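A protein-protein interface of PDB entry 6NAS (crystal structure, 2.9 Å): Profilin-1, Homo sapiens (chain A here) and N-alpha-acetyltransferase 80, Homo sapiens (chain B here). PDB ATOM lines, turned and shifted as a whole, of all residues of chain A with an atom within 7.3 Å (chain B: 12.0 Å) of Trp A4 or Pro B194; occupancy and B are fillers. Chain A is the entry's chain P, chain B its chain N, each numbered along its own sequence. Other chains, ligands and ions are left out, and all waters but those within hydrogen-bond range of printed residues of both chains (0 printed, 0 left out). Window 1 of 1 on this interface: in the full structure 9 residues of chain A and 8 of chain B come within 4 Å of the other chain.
Of chain B, only Pro B193 (3.5 Å) comes within 4 Å of Gly A3.
Trp A4 touches four residues of chain B.
No residue of chain B comes within 4 Å of Asn A5.
No residue of chain B comes within 4 Å of Ala A6.
Printed residues of chain B within 4 Å of Tyr A7: Pro B194 and Pro B195.
No residue of chain B comes within 4 Å of Ile A8.
Of the printed residues of chain B, Asn A10 touches Leu B196 (2.9 Å).
No residue of chain B comes within 4 Å of Ile A22.
Trp A32 touches just one residue of chain B: Pro B191 (3.6 Å).
No residue of chain B comes within 4 Å of Ala A33.
Met A131 touches none of the printed residues of chain B.
Leu A135 touches just one residue of chain B: Pro B194.
Of chain B, only Pro B194 (3.6 Å) comes within 4 Å of Ser A138.
Tyr A140 touches just these residues of chain B: Pro B191, Pro B192 and Pro B194.
Of the printed residues of chain A, Pro B191 touches Trp A4 (2.8 Å), Trp A32 (3.6 Å) and Tyr A140 (3.3 Å).
Pro B194 touches just these residues of chain A: Trp A4, Tyr A7, Leu A135, Ser A138 and Tyr A140.
Printed residues of chain A within 4 Å of Pro B195: Tyr A7 (3.4 Å) and His A134 (2.7 Å).
Printed residues of chain A within 4 Å of Leu B196: Asn A10 and His A134.
The nearest residue of chain B that does not touch Trp A4 is Pro B192 (4.2 Å).
The nearest residue of chain A that does not touch Pro B194 is His A134 (5.1 Å).
The nearest printed residue of chain A that does not touch Pro B191 is Lys A108 (4.7 Å).
The side-chain hydroxyl (OH) of Tyr A7 sits at hydrogen-bond distance from a ring nitrogen (NE2) of His A134, 3.0 Å away.
N of Trp A32 is in hydrogen-bond range of O of Ile A22 (2.9 Å).
The backbone NH (N) of Lys A108 sits at hydrogen-bond distance from the chain-end carboxylate (O) of Tyr A140, at 3.3 Å.
The backbone carbonyl oxygen (O) of His A134 lies within hydrogen-bond range of the side-chain hydroxyl (OG) of Ser A138 (3.1 Å).
The backbone carbonyl oxygen (O) of Leu A135 sits at hydrogen-bond distance from the backbone NH (N) of Tyr A140 (2.6 Å).
Hydrophobic or aromatic side chains of chain B that line the printed part of chain A: Leu B190, Pro B191, Pro B192, Pro B193, Pro B194, Leu B196 and Pro B197.
Of the 22 printed residues of chain A, 9 touch a printed residue of chain B.
Printed residues of chain A that touch a printed residue of chain B: Gly A3, Trp A4, Tyr A7, Asn A10, Trp A32, His A134, Leu A135, Ser A138 and Tyr A140.
Among the printed residues, 17 pairs touch across the chains.
Among the printed residues, no Asp or Glu carboxylate lies within 4 Å of a Lys or Arg side-chain nitrogen of the other chain.
Pro B193 touches Gly A3.
Leu B190 touches Trp A4 (CD2 to CD1, 3.5 Å).
Trp A4 touches Pro B193 (N to CG, 3.5 Å).
Asn A10 touches Leu B196.
Pro B191 touches Trp A32 (CD to CH2, 3.6 Å).
CE1 of His A134 touches C of Leu B196, 3.9 Å away.
Leu A135 touches Pro B194.
CB of Pro B194 touches CB of Ser A138, 3.6 Å away.
Tyr A140 touches Pro B191.
Pro B194 touches Tyr A140 (CD to CE1, 3.9 Å).
The backbone carbonyl oxygen (O) of Pro B191 lies within hydrogen-bond range of the indole nitrogen (NE1) of Trp A4 (2.8 Å).
The backbone carbonyl oxygen of Pro B192 lies within hydrogen-bond range of the side-chain hydroxyl of Tyr A140 (2.7 Å).
The backbone carbonyl oxygen (O) of Pro B194 is in hydrogen-bond range of the side-chain hydroxyl (OH) of Tyr A7.
The backbone carbonyl oxygen of Pro B195 sits at hydrogen-bond distance from the side-chain hydroxyl of Tyr A7, 3.4 Å away.
A ring nitrogen (NE2) of His A134 lies within hydrogen-bond range of the backbone carbonyl oxygen (O) of Pro B195, at 2.7 Å.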
ATOM      1  N   GLY A   3       9.207  21.629 -26.042  1.00  0.00           N
ATOM      2  CA  GLY A   3       8.005  20.970 -25.568  1.00  0.00           C
ATOM      3  C   GLY A   3       8.086  19.457 -25.635  1.00  0.00           C
ATOM      4  O   GLY A   3       9.121  18.871 -25.319  1.00  0.00           O
ATOM      5  N   TRP A   4       6.980  18.819 -26.029  1.00  0.00           N
ATOM      6  CA  TRP A   4       6.991  17.369 -26.184  1.00  0.00           C
ATOM      7  C   TRP A   4       7.984  16.931 -27.248  1.00  0.00           C
ATOM      8  O   TRP A   4       8.603  15.868 -27.118  1.00  0.00           O
ATOM      9  CB  TRP A   4       5.587  16.864 -26.530  1.00  0.00           C
ATOM     10  CG  TRP A   4       4.709  16.646 -25.334  1.00  0.00           C
ATOM     11  CD1 TRP A   4       3.528  17.269 -25.054  1.00  0.00           C
ATOM     12  CD2 TRP A   4       4.952  15.739 -24.251  1.00  0.00           C
ATOM     13  NE1 TRP A   4       3.018  16.803 -23.865  1.00  0.00           N
ATOM     14  CE2 TRP A   4       3.875  15.865 -23.352  1.00  0.00           C
ATOM     15  CE3 TRP A   4       5.977  14.836 -23.955  1.00  0.00           C
ATOM     16  CZ2 TRP A   4       3.793  15.119 -22.177  1.00  0.00           C
ATOM     17  CZ3 TRP A   4       5.895  14.097 -22.788  1.00  0.00           C
ATOM     18  CH2 TRP A   4       4.810  14.244 -21.914  1.00  0.00           C
ATOM     19  N   ASN A   5       8.154  17.732 -28.302  1.00  0.00           N
ATOM     20  CA  ASN A   5       9.153  17.428 -29.316  1.00  0.00           C
ATOM     21  C   ASN A   5      10.554  17.374 -28.734  1.00  0.00           C
ATOM     22  O   ASN A   5      11.417  16.690 -29.298  1.00  0.00           O
ATOM     23  CB  ASN A   5       9.088  18.471 -30.434  1.00  0.00           C
ATOM     24  CG  ASN A   5       7.960  18.209 -31.410  1.00  0.00           C
ATOM     25  OD1 ASN A   5       8.131  17.485 -32.389  1.00  0.00           O
ATOM     26  ND2 ASN A   5       6.798  18.798 -31.146  1.00  0.00           N
ATOM     27  N   ALA A   6      10.800  18.084 -27.629  1.00  0.00           N
ATOM     28  CA  ALA A   6      12.091  18.020 -26.961  1.00  0.00           C
ATOM     29  C   ALA A   6      12.372  16.661 -26.361  1.00  0.00           C
ATOM     30  O   ALA A   6      13.471  16.442 -25.834  1.00  0.00           O
ATOM     31  CB  ALA A   6      12.171  19.108 -25.887  1.00  0.00           C
ATOM     32  N   TYR A   7      11.410  15.753 -26.421  1.00  0.00           N
ATOM     33  CA  TYR A   7      11.632  14.369 -26.035  1.00  0.00           C
ATOM     34  C   TYR A   7      12.000  13.506 -27.231  1.00  0.00           C
ATOM     35  O   TYR A   7      12.913  12.679 -27.137  1.00  0.00           O
ATOM     36  CB  TYR A   7      10.388  13.803 -25.354  1.00  0.00           C
ATOM     37  CG  TYR A   7      10.358  14.054 -23.867  1.00  0.00           C
ATOM     38  CD1 TYR A   7      10.778  15.268 -23.345  1.00  0.00           C
ATOM     39  CD2 TYR A   7       9.907  13.083 -22.986  1.00  0.00           C
ATOM     40  CE1 TYR A   7      10.754  15.507 -21.987  1.00  0.00           C
ATOM     41  CE2 TYR A   7       9.875  13.313 -21.629  1.00  0.00           C
ATOM     42  CZ  TYR A   7      10.299  14.529 -21.134  1.00  0.00           C
ATOM     43  OH  TYR A   7      10.269  14.760 -19.779  1.00  0.00           O
ATOM     44  N   ILE A   8      11.300  13.682 -28.355  1.00  0.00           N
ATOM     45  CA  ILE A   8      11.672  12.973 -29.576  1.00  0.00           C
ATOM     46  C   ILE A   8      13.168  13.121 -29.824  1.00  0.00           C
ATOM     47  O   ILE A   8      13.881  12.137 -30.051  1.00  0.00           O
ATOM     48  CB  ILE A   8      10.847  13.488 -30.769  1.00  0.00           C
ATOM     49  CG1 ILE A   8       9.348  13.385 -30.468  1.00  0.00           C
ATOM     50  CG2 ILE A   8      11.198  12.714 -32.027  1.00  0.00           C
ATOM     51  CD1 ILE A   8       8.886  12.010 -30.022  1.00  0.00           C
ATOM     52  N   ASP A   9      13.668  14.357 -29.754  1.00  0.00           N
ATOM     53  CA  ASP A   9      15.101  14.573 -29.914  1.00  0.00           C
ATOM     54  C   ASP A   9      15.886  13.924 -28.781  1.00  0.00           C
ATOM     55  O   ASP A   9      16.910  13.274 -29.022  1.00  0.00           O
ATOM     56  CB  ASP A   9      15.408  16.070 -29.986  1.00  0.00           C
ATOM     57  CG  ASP A   9      14.998  16.688 -31.311  1.00  0.00           C
ATOM     58  OD1 ASP A   9      14.711  15.928 -32.260  1.00  0.00           O
ATOM     59  OD2 ASP A   9      14.951  17.933 -31.399  1.00  0.00           O
ATOM     60  N   ASN A  10      15.420  14.081 -27.540  1.00  0.00           N
ATOM     61  CA  ASN A  10      16.107  13.453 -26.419  1.00  0.00           C
ATOM     62  C   ASN A  10      16.144  11.936 -26.559  1.00  0.00           C
ATOM     63  O   ASN A  10      16.979  11.285 -25.919  1.00  0.00           O
ATOM     64  CB  ASN A  10      15.439  13.844 -25.101  1.00  0.00           C
ATOM     65  CG  ASN A  10      16.354  13.648 -23.903  1.00  0.00           C
ATOM     66  OD1 ASN A  10      16.952  14.599 -23.402  1.00  0.00           O
ATOM     67  ND2 ASN A  10      16.470  12.406 -23.444  1.00  0.00           N
ATOM     68  N   ILE A  22       5.646   9.952 -28.729  1.00  0.00           N
ATOM     69  CA  ILE A  22       4.862   9.976 -27.501  1.00  0.00           C
ATOM     70  C   ILE A  22       3.398  10.089 -27.907  1.00  0.00           C
ATOM     71  O   ILE A  22       3.028  11.000 -28.657  1.00  0.00           O
ATOM     72  CB  ILE A  22       5.262  11.146 -26.585  1.00  0.00           C
ATOM     73  CG1 ILE A  22       6.742  11.051 -26.204  1.00  0.00           C
ATOM     74  CG2 ILE A  22       4.383  11.168 -25.341  1.00  0.00           C
ATOM     75  CD1 ILE A  22       7.091   9.845 -25.364  1.00  0.00           C
ATOM     76  N   TRP A  32       1.083  12.876 -29.604  1.00  0.00           N
ATOM     77  CA  TRP A  32       1.540  14.145 -29.046  1.00  0.00           C
ATOM     78  C   TRP A  32       2.817  14.629 -29.725  1.00  0.00           C
ATOM     79  O   TRP A  32       2.954  15.821 -30.021  1.00  0.00           O
ATOM     80  CB  TRP A  32       1.764  14.010 -27.539  1.00  0.00           C
ATOM     81  CG  TRP A  32       0.515  13.719 -26.773  1.00  0.00           C
ATOM     82  CD1 TRP A  32      -0.729  13.494 -27.286  1.00  0.00           C
ATOM     83  CD2 TRP A  32       0.383  13.621 -25.349  1.00  0.00           C
ATOM     84  NE1 TRP A  32      -1.626  13.261 -26.274  1.00  0.00           N
ATOM     85  CE2 TRP A  32      -0.969  13.334 -25.074  1.00  0.00           C
ATOM     86  CE3 TRP A  32       1.276  13.749 -24.282  1.00  0.00           C
ATOM     87  CZ2 TRP A  32      -1.448  13.171 -23.776  1.00  0.00           C
ATOM     88  CZ3 TRP A  32       0.798  13.588 -22.994  1.00  0.00           C
ATOM     89  CH2 TRP A  32      -0.551  13.302 -22.752  1.00  0.00           C
ATOM     90  N   ALA A  33       3.762  13.725 -29.969  1.00  0.00           N
ATOM     91  CA  ALA A  33       5.010  14.077 -30.626  1.00  0.00           C
ATOM     92  C   ALA A  33       5.543  12.854 -31.353  1.00  0.00           C
ATOM     93  O   ALA A  33       5.381  11.721 -30.892  1.00  0.00           O
ATOM     94  CB  ALA A  33       6.048  14.598 -29.625  1.00  0.00           C
ATOM     95  N   ALA A  34       6.180  13.092 -32.496  1.00  0.00           N
ATOM     96  CA  ALA A  34       6.738  12.005 -33.289  1.00  0.00           C
ATOM     97  C   ALA A  34       7.752  12.577 -34.269  1.00  0.00           C
ATOM     98  O   ALA A  34       7.767  13.779 -34.547  1.00  0.00           O
ATOM     99  CB  ALA A  34       5.643  11.236 -34.037  1.00  0.00           C
ATOM    100  N   LYS A 108      -0.327   8.142 -18.718  1.00  0.00           N
ATOM    101  CA  LYS A 108      -1.101   8.722 -19.809  1.00  0.00           C
ATOM    102  C   LYS A 108      -0.470   8.580 -21.186  1.00  0.00           C
ATOM    103  O   LYS A 108      -1.098   8.988 -22.164  1.00  0.00           O
ATOM    104  CB  LYS A 108      -1.356  10.222 -19.543  1.00  0.00           C
ATOM    105  CG  LYS A 108      -2.298  10.518 -18.401  1.00  0.00           C
ATOM    106  CD  LYS A 108      -1.657  11.423 -17.339  1.00  0.00           C
ATOM    107  CE  LYS A 108      -0.972  12.639 -17.952  1.00  0.00           C
ATOM    108  NZ  LYS A 108      -1.036  13.837 -17.074  1.00  0.00           N
ATOM    109  N   THR A 109       0.696   7.992 -21.383  1.00  0.00           N
ATOM    110  CA  THR A 109       1.324   8.049 -22.689  1.00  0.00           C
ATOM    111  C   THR A 109       1.868   6.683 -23.040  1.00  0.00           C
ATOM    112  O   THR A 109       2.181   5.923 -22.154  1.00  0.00           O
ATOM    113  CB  THR A 109       2.578   8.924 -22.693  1.00  0.00           C
ATOM    114  OG1 THR A 109       3.480   8.333 -21.770  1.00  0.00           O
ATOM    115  CG2 THR A 109       2.316  10.354 -22.301  1.00  0.00           C
ATOM    116  N   MET A 131      12.854   6.104 -20.406  1.00  0.00           N
ATOM    117  CA  MET A 131      12.006   7.260 -20.685  1.00  0.00           C
ATOM    118  C   MET A 131      10.659   7.125 -19.988  1.00  0.00           C
ATOM    119  O   MET A 131      10.148   8.091 -19.411  1.00  0.00           O
ATOM    120  CB  MET A 131      11.817   7.415 -22.193  1.00  0.00           C
ATOM    121  CG  MET A 131      11.075   8.679 -22.620  1.00  0.00           C
ATOM    122  SD  MET A 131      12.028  10.203 -22.441  1.00  0.00           S
ATOM    123  CE  MET A 131      11.682  10.652 -20.741  1.00  0.00           C
ATOM    124  N   HIS A 134      11.001   7.778 -16.274  1.00  0.00           N
ATOM    125  CA  HIS A 134      11.114   9.206 -16.002  1.00  0.00           C
ATOM    126  C   HIS A 134       9.742   9.864 -15.963  1.00  0.00           C
ATOM    127  O   HIS A 134       9.443  10.650 -15.057  1.00  0.00           O
ATOM    128  CB  HIS A 134      11.995   9.872 -17.059  1.00  0.00           C
ATOM    129  CG  HIS A 134      11.947  11.368 -17.027  1.00  0.00           C
ATOM    130  ND1 HIS A 134      12.473  12.107 -15.990  1.00  0.00           N
ATOM    131  CD2 HIS A 134      11.430  12.263 -17.902  1.00  0.00           C
ATOM    132  CE1 HIS A 134      12.285  13.392 -16.229  1.00  0.00           C
ATOM    133  NE2 HIS A 134      11.655  13.514 -17.383  1.00  0.00           N
ATOM    134  N   LEU A 135       8.888   9.554 -16.940  1.00  0.00           N
ATOM    135  CA  LEU A 135       7.585  10.207 -17.017  1.00  0.00           C
ATOM    136  C   LEU A 135       6.606   9.652 -15.989  1.00  0.00           C
ATOM    137  O   LEU A 135       5.756  10.400 -15.494  1.00  0.00           O
ATOM    138  CB  LEU A 135       7.015  10.077 -18.430  1.00  0.00           C
ATOM    139  CG  LEU A 135       7.725  10.943 -19.474  1.00  0.00           C
ATOM    140  CD1 LEU A 135       7.102  10.778 -20.852  1.00  0.00           C
ATOM    141  CD2 LEU A 135       7.712  12.415 -19.066  1.00  0.00           C
ATOM    142  N   ARG A 136       6.699   8.363 -15.654  1.00  0.00           N
ATOM    143  CA  ARG A 136       5.964   7.859 -14.497  1.00  0.00           C
ATOM    144  C   ARG A 136       6.401   8.593 -13.234  1.00  0.00           C
ATOM    145  O   ARG A 136       5.568   9.011 -12.421  1.00  0.00           O
ATOM    146  CB  ARG A 136       6.182   6.355 -14.340  1.00  0.00           C
ATOM    147  CG  ARG A 136       5.290   5.484 -15.214  1.00  0.00           C
ATOM    148  CD  ARG A 136       5.642   4.011 -15.034  1.00  0.00           C
ATOM    149  NE  ARG A 136       6.147   3.411 -16.268  1.00  0.00           N
ATOM    150  CZ  ARG A 136       6.973   2.369 -16.317  1.00  0.00           C
ATOM    151  NH1 ARG A 136       7.372   1.894 -17.490  1.00  0.00           N
ATOM    152  NH2 ARG A 136       7.411   1.807 -15.199  1.00  0.00           N
ATOM    153  N   ARG A 137       7.717   8.760 -13.060  1.00  0.00           N
ATOM    154  CA  ARG A 137       8.233   9.518 -11.926  1.00  0.00           C
ATOM    155  C   ARG A 137       7.605  10.901 -11.848  1.00  0.00           C
ATOM    156  O   ARG A 137       7.431  11.445 -10.753  1.00  0.00           O
ATOM    157  CB  ARG A 137       9.755   9.646 -12.024  1.00  0.00           C
ATOM    158  CG  ARG A 137      10.521   8.682 -11.136  1.00  0.00           C
ATOM    159  CD  ARG A 137      11.882   9.242 -10.745  1.00  0.00           C
ATOM    160  NE  ARG A 137      12.762   9.445 -11.892  1.00  0.00           N
ATOM    161  CZ  ARG A 137      13.331   8.460 -12.580  1.00  0.00           C
ATOM    162  NH1 ARG A 137      14.126   8.739 -13.605  1.00  0.00           N
ATOM    163  NH2 ARG A 137      13.098   7.196 -12.255  1.00  0.00           N
ATOM    164  N   SER A 138       7.263  11.490 -12.993  1.00  0.00           N
ATOM    165  CA  SER A 138       6.591  12.780 -13.042  1.00  0.00           C
ATOM    166  C   SER A 138       5.079  12.632 -13.179  1.00  0.00           C
ATOM    167  O   SER A 138       4.408  13.566 -13.629  1.00  0.00           O
ATOM    168  CB  SER A 138       7.152  13.618 -14.190  1.00  0.00           C
ATOM    169  OG  SER A 138       8.564  13.501 -14.258  1.00  0.00           O
ATOM    170  N   GLN A 139       4.535  11.474 -12.803  1.00  0.00           N
ATOM    171  CA  GLN A 139       3.092  11.227 -12.829  1.00  0.00           C
ATOM    172  C   GLN A 139       2.512  11.417 -14.229  1.00  0.00           C
ATOM    173  O   GLN A 139       1.387  11.891 -14.401  1.00  0.00           O
ATOM    174  CB  GLN A 139       2.369  12.109 -11.811  1.00  0.00           C
ATOM    175  CG  GLN A 139       2.103  11.418 -10.477  1.00  0.00           C
ATOM    176  CD  GLN A 139       0.735  10.759 -10.427  1.00  0.00           C
ATOM    177  OE1 GLN A 139      -0.226  11.253 -11.019  1.00  0.00           O
ATOM    178  NE2 GLN A 139       0.640   9.639  -9.716  1.00  0.00           N
ATOM    179  N   TYR A 140       3.284  11.031 -15.240  1.00  0.00           N
ATOM    180  CA  TYR A 140       2.793  10.966 -16.613  1.00  0.00           C
ATOM    181  C   TYR A 140       2.853   9.525 -17.112  1.00  0.00           C
ATOM    182  O   TYR A 140       2.717   9.263 -18.308  1.00  0.00           O
ATOM    183  CB  TYR A 140       3.605  11.871 -17.536  1.00  0.00           C
ATOM    184  CG  TYR A 140       3.015  13.253 -17.701  1.00  0.00           C
ATOM    185  CD1 TYR A 140       3.162  14.212 -16.710  1.00  0.00           C
ATOM    186  CD2 TYR A 140       2.304  13.597 -18.845  1.00  0.00           C
ATOM    187  CE1 TYR A 140       2.624  15.475 -16.852  1.00  0.00           C
ATOM    188  CE2 TYR A 140       1.763  14.859 -18.996  1.00  0.00           C
ATOM    189  CZ  TYR A 140       1.924  15.794 -17.995  1.00  0.00           C
ATOM    190  OH  TYR A 140       1.392  17.055 -18.135  1.00  0.00           O
ATOM    191  OXT TYR A 140       3.046   8.589 -16.332  1.00  0.00           O
ATOM    192  N   LEU B 190      -3.854  18.515 -24.625  1.00  0.00           N
ATOM    193  CA  LEU B 190      -2.435  18.201 -24.772  1.00  0.00           C
ATOM    194  C   LEU B 190      -1.652  18.831 -23.622  1.00  0.00           C
ATOM    195  O   LEU B 190      -1.170  19.956 -23.741  1.00  0.00           O
ATOM    196  CB  LEU B 190      -1.918  18.701 -26.121  1.00  0.00           C
ATOM    197  CG  LEU B 190      -0.700  17.969 -26.687  1.00  0.00           C
ATOM    198  CD1 LEU B 190      -0.798  17.866 -28.205  1.00  0.00           C
ATOM    199  CD2 LEU B 190       0.590  18.663 -26.283  1.00  0.00           C
ATOM    200  N   PRO B 191      -1.517  18.107 -22.511  1.00  0.00           N
ATOM    201  CA  PRO B 191      -0.917  18.707 -21.310  1.00  0.00           C
ATOM    202  C   PRO B 191       0.558  18.992 -21.524  1.00  0.00           C
ATOM    203  O   PRO B 191       1.182  18.439 -22.441  1.00  0.00           O
ATOM    204  CB  PRO B 191      -1.131  17.644 -20.218  1.00  0.00           C
ATOM    205  CG  PRO B 191      -1.815  16.476 -20.878  1.00  0.00           C
ATOM    206  CD  PRO B 191      -1.710  16.653 -22.363  1.00  0.00           C
ATOM    207  N   PRO B 192       1.149  19.846 -20.694  1.00  0.00           N
ATOM    208  CA  PRO B 192       2.542  20.264 -20.918  1.00  0.00           C
ATOM    209  C   PRO B 192       3.518  19.205 -20.443  1.00  0.00           C
ATOM    210  O   PRO B 192       3.260  18.507 -19.451  1.00  0.00           O
ATOM    211  CB  PRO B 192       2.658  21.552 -20.089  1.00  0.00           C
ATOM    212  CG  PRO B 192       1.661  21.375 -18.982  1.00  0.00           C
ATOM    213  CD  PRO B 192       0.546  20.494 -19.512  1.00  0.00           C
ATOM    214  N   PRO B 193       4.650  19.053 -21.125  1.00  0.00           N
ATOM    215  CA  PRO B 193       5.618  18.013 -20.741  1.00  0.00           C
ATOM    216  C   PRO B 193       6.336  18.369 -19.452  1.00  0.00           C
ATOM    217  O   PRO B 193       6.685  19.537 -19.228  1.00  0.00           O
ATOM    218  CB  PRO B 193       6.590  17.977 -21.932  1.00  0.00           C
ATOM    219  CG  PRO B 193       6.479  19.332 -22.560  1.00  0.00           C
ATOM    220  CD  PRO B 193       5.054  19.772 -22.352  1.00  0.00           C
ATOM    221  N   PRO B 194       6.571  17.391 -18.579  1.00  0.00           N
ATOM    222  CA  PRO B 194       7.409  17.640 -17.397  1.00  0.00           C
ATOM    223  C   PRO B 194       8.842  17.927 -17.804  1.00  0.00           C
ATOM    224  O   PRO B 194       9.162  17.948 -19.004  1.00  0.00           O
ATOM    225  CB  PRO B 194       7.298  16.334 -16.594  1.00  0.00           C
ATOM    226  CG  PRO B 194       6.880  15.300 -17.588  1.00  0.00           C
ATOM    227  CD  PRO B 194       6.033  16.017 -18.602  1.00  0.00           C
ATOM    228  N   PRO B 195       9.739  18.150 -16.847  1.00  0.00           N
ATOM    229  CA  PRO B 195      11.104  18.548 -17.202  1.00  0.00           C
ATOM    230  C   PRO B 195      11.961  17.374 -17.647  1.00  0.00           C
ATOM    231  O   PRO B 195      11.814  16.244 -17.177  1.00  0.00           O
ATOM    232  CB  PRO B 195      11.655  19.157 -15.901  1.00  0.00           C
ATOM    233  CG  PRO B 195      10.514  19.124 -14.896  1.00  0.00           C
ATOM    234  CD  PRO B 195       9.545  18.096 -15.387  1.00  0.00           C
ATOM    235  N   LEU B 196      12.877  17.670 -18.569  1.00  0.00           N
ATOM    236  CA  LEU B 196      13.901  16.732 -19.005  1.00  0.00           C
ATOM    237  C   LEU B 196      14.571  16.063 -17.812  1.00  0.00           C
ATOM    238  O   LEU B 196      14.507  16.588 -16.694  1.00  0.00           O
ATOM    239  CB  LEU B 196      14.969  17.459 -19.828  1.00  0.00           C
ATOM    240  CG  LEU B 196      14.786  17.659 -21.327  1.00  0.00           C
ATOM    241  CD1 LEU B 196      15.645  18.824 -21.803  1.00  0.00           C
ATOM    242  CD2 LEU B 196      15.150  16.390 -22.071  1.00  0.00           C
ATOM    243  N   PRO B 197      15.220  14.905 -17.995  1.00  0.00           N
ATOM    244  CA  PRO B 197      16.221  14.475 -17.004  1.00  0.00           C
ATOM    245  C   PRO B 197      17.289  15.554 -16.882  1.00  0.00           C
ATOM    246  O   PRO B 197      18.237  15.589 -17.674  1.00  0.00           O
ATOM    247  CB  PRO B 197      16.763  13.159 -17.573  1.00  0.00           C
ATOM    248  CG  PRO B 197      16.271  13.087 -18.994  1.00  0.00           C
ATOM    249  CD  PRO B 197      15.007  13.899 -19.052  1.00  0.00           C
ATOM    250  N   GLU B 198      17.128  16.432 -15.891  1.00  0.00           N
ATOM    251  CA  GLU B 198      17.765  17.751 -15.850  1.00  0.00           C
ATOM    252  C   GLU B 198      18.375  18.166 -17.186  1.00  0.00           C
ATOM    253  O   GLU B 198      19.591  18.156 -17.361  1.00  0.00           O
ATOM    254  CB  GLU B 198      18.836  17.799 -14.751  1.00  0.00           C
ATOM    255  CG  GLU B 198      18.277  17.655 -13.338  1.00  0.00           C
ATOM    256  CD  GLU B 198      19.350  17.717 -12.264  1.00  0.00           C
ATOM    257  OE1 GLU B 198      20.537  17.901 -12.611  1.00  0.00           O
ATOM    258  OE2 GLU B 198      19.002  17.582 -11.071  1.00  0.00           O
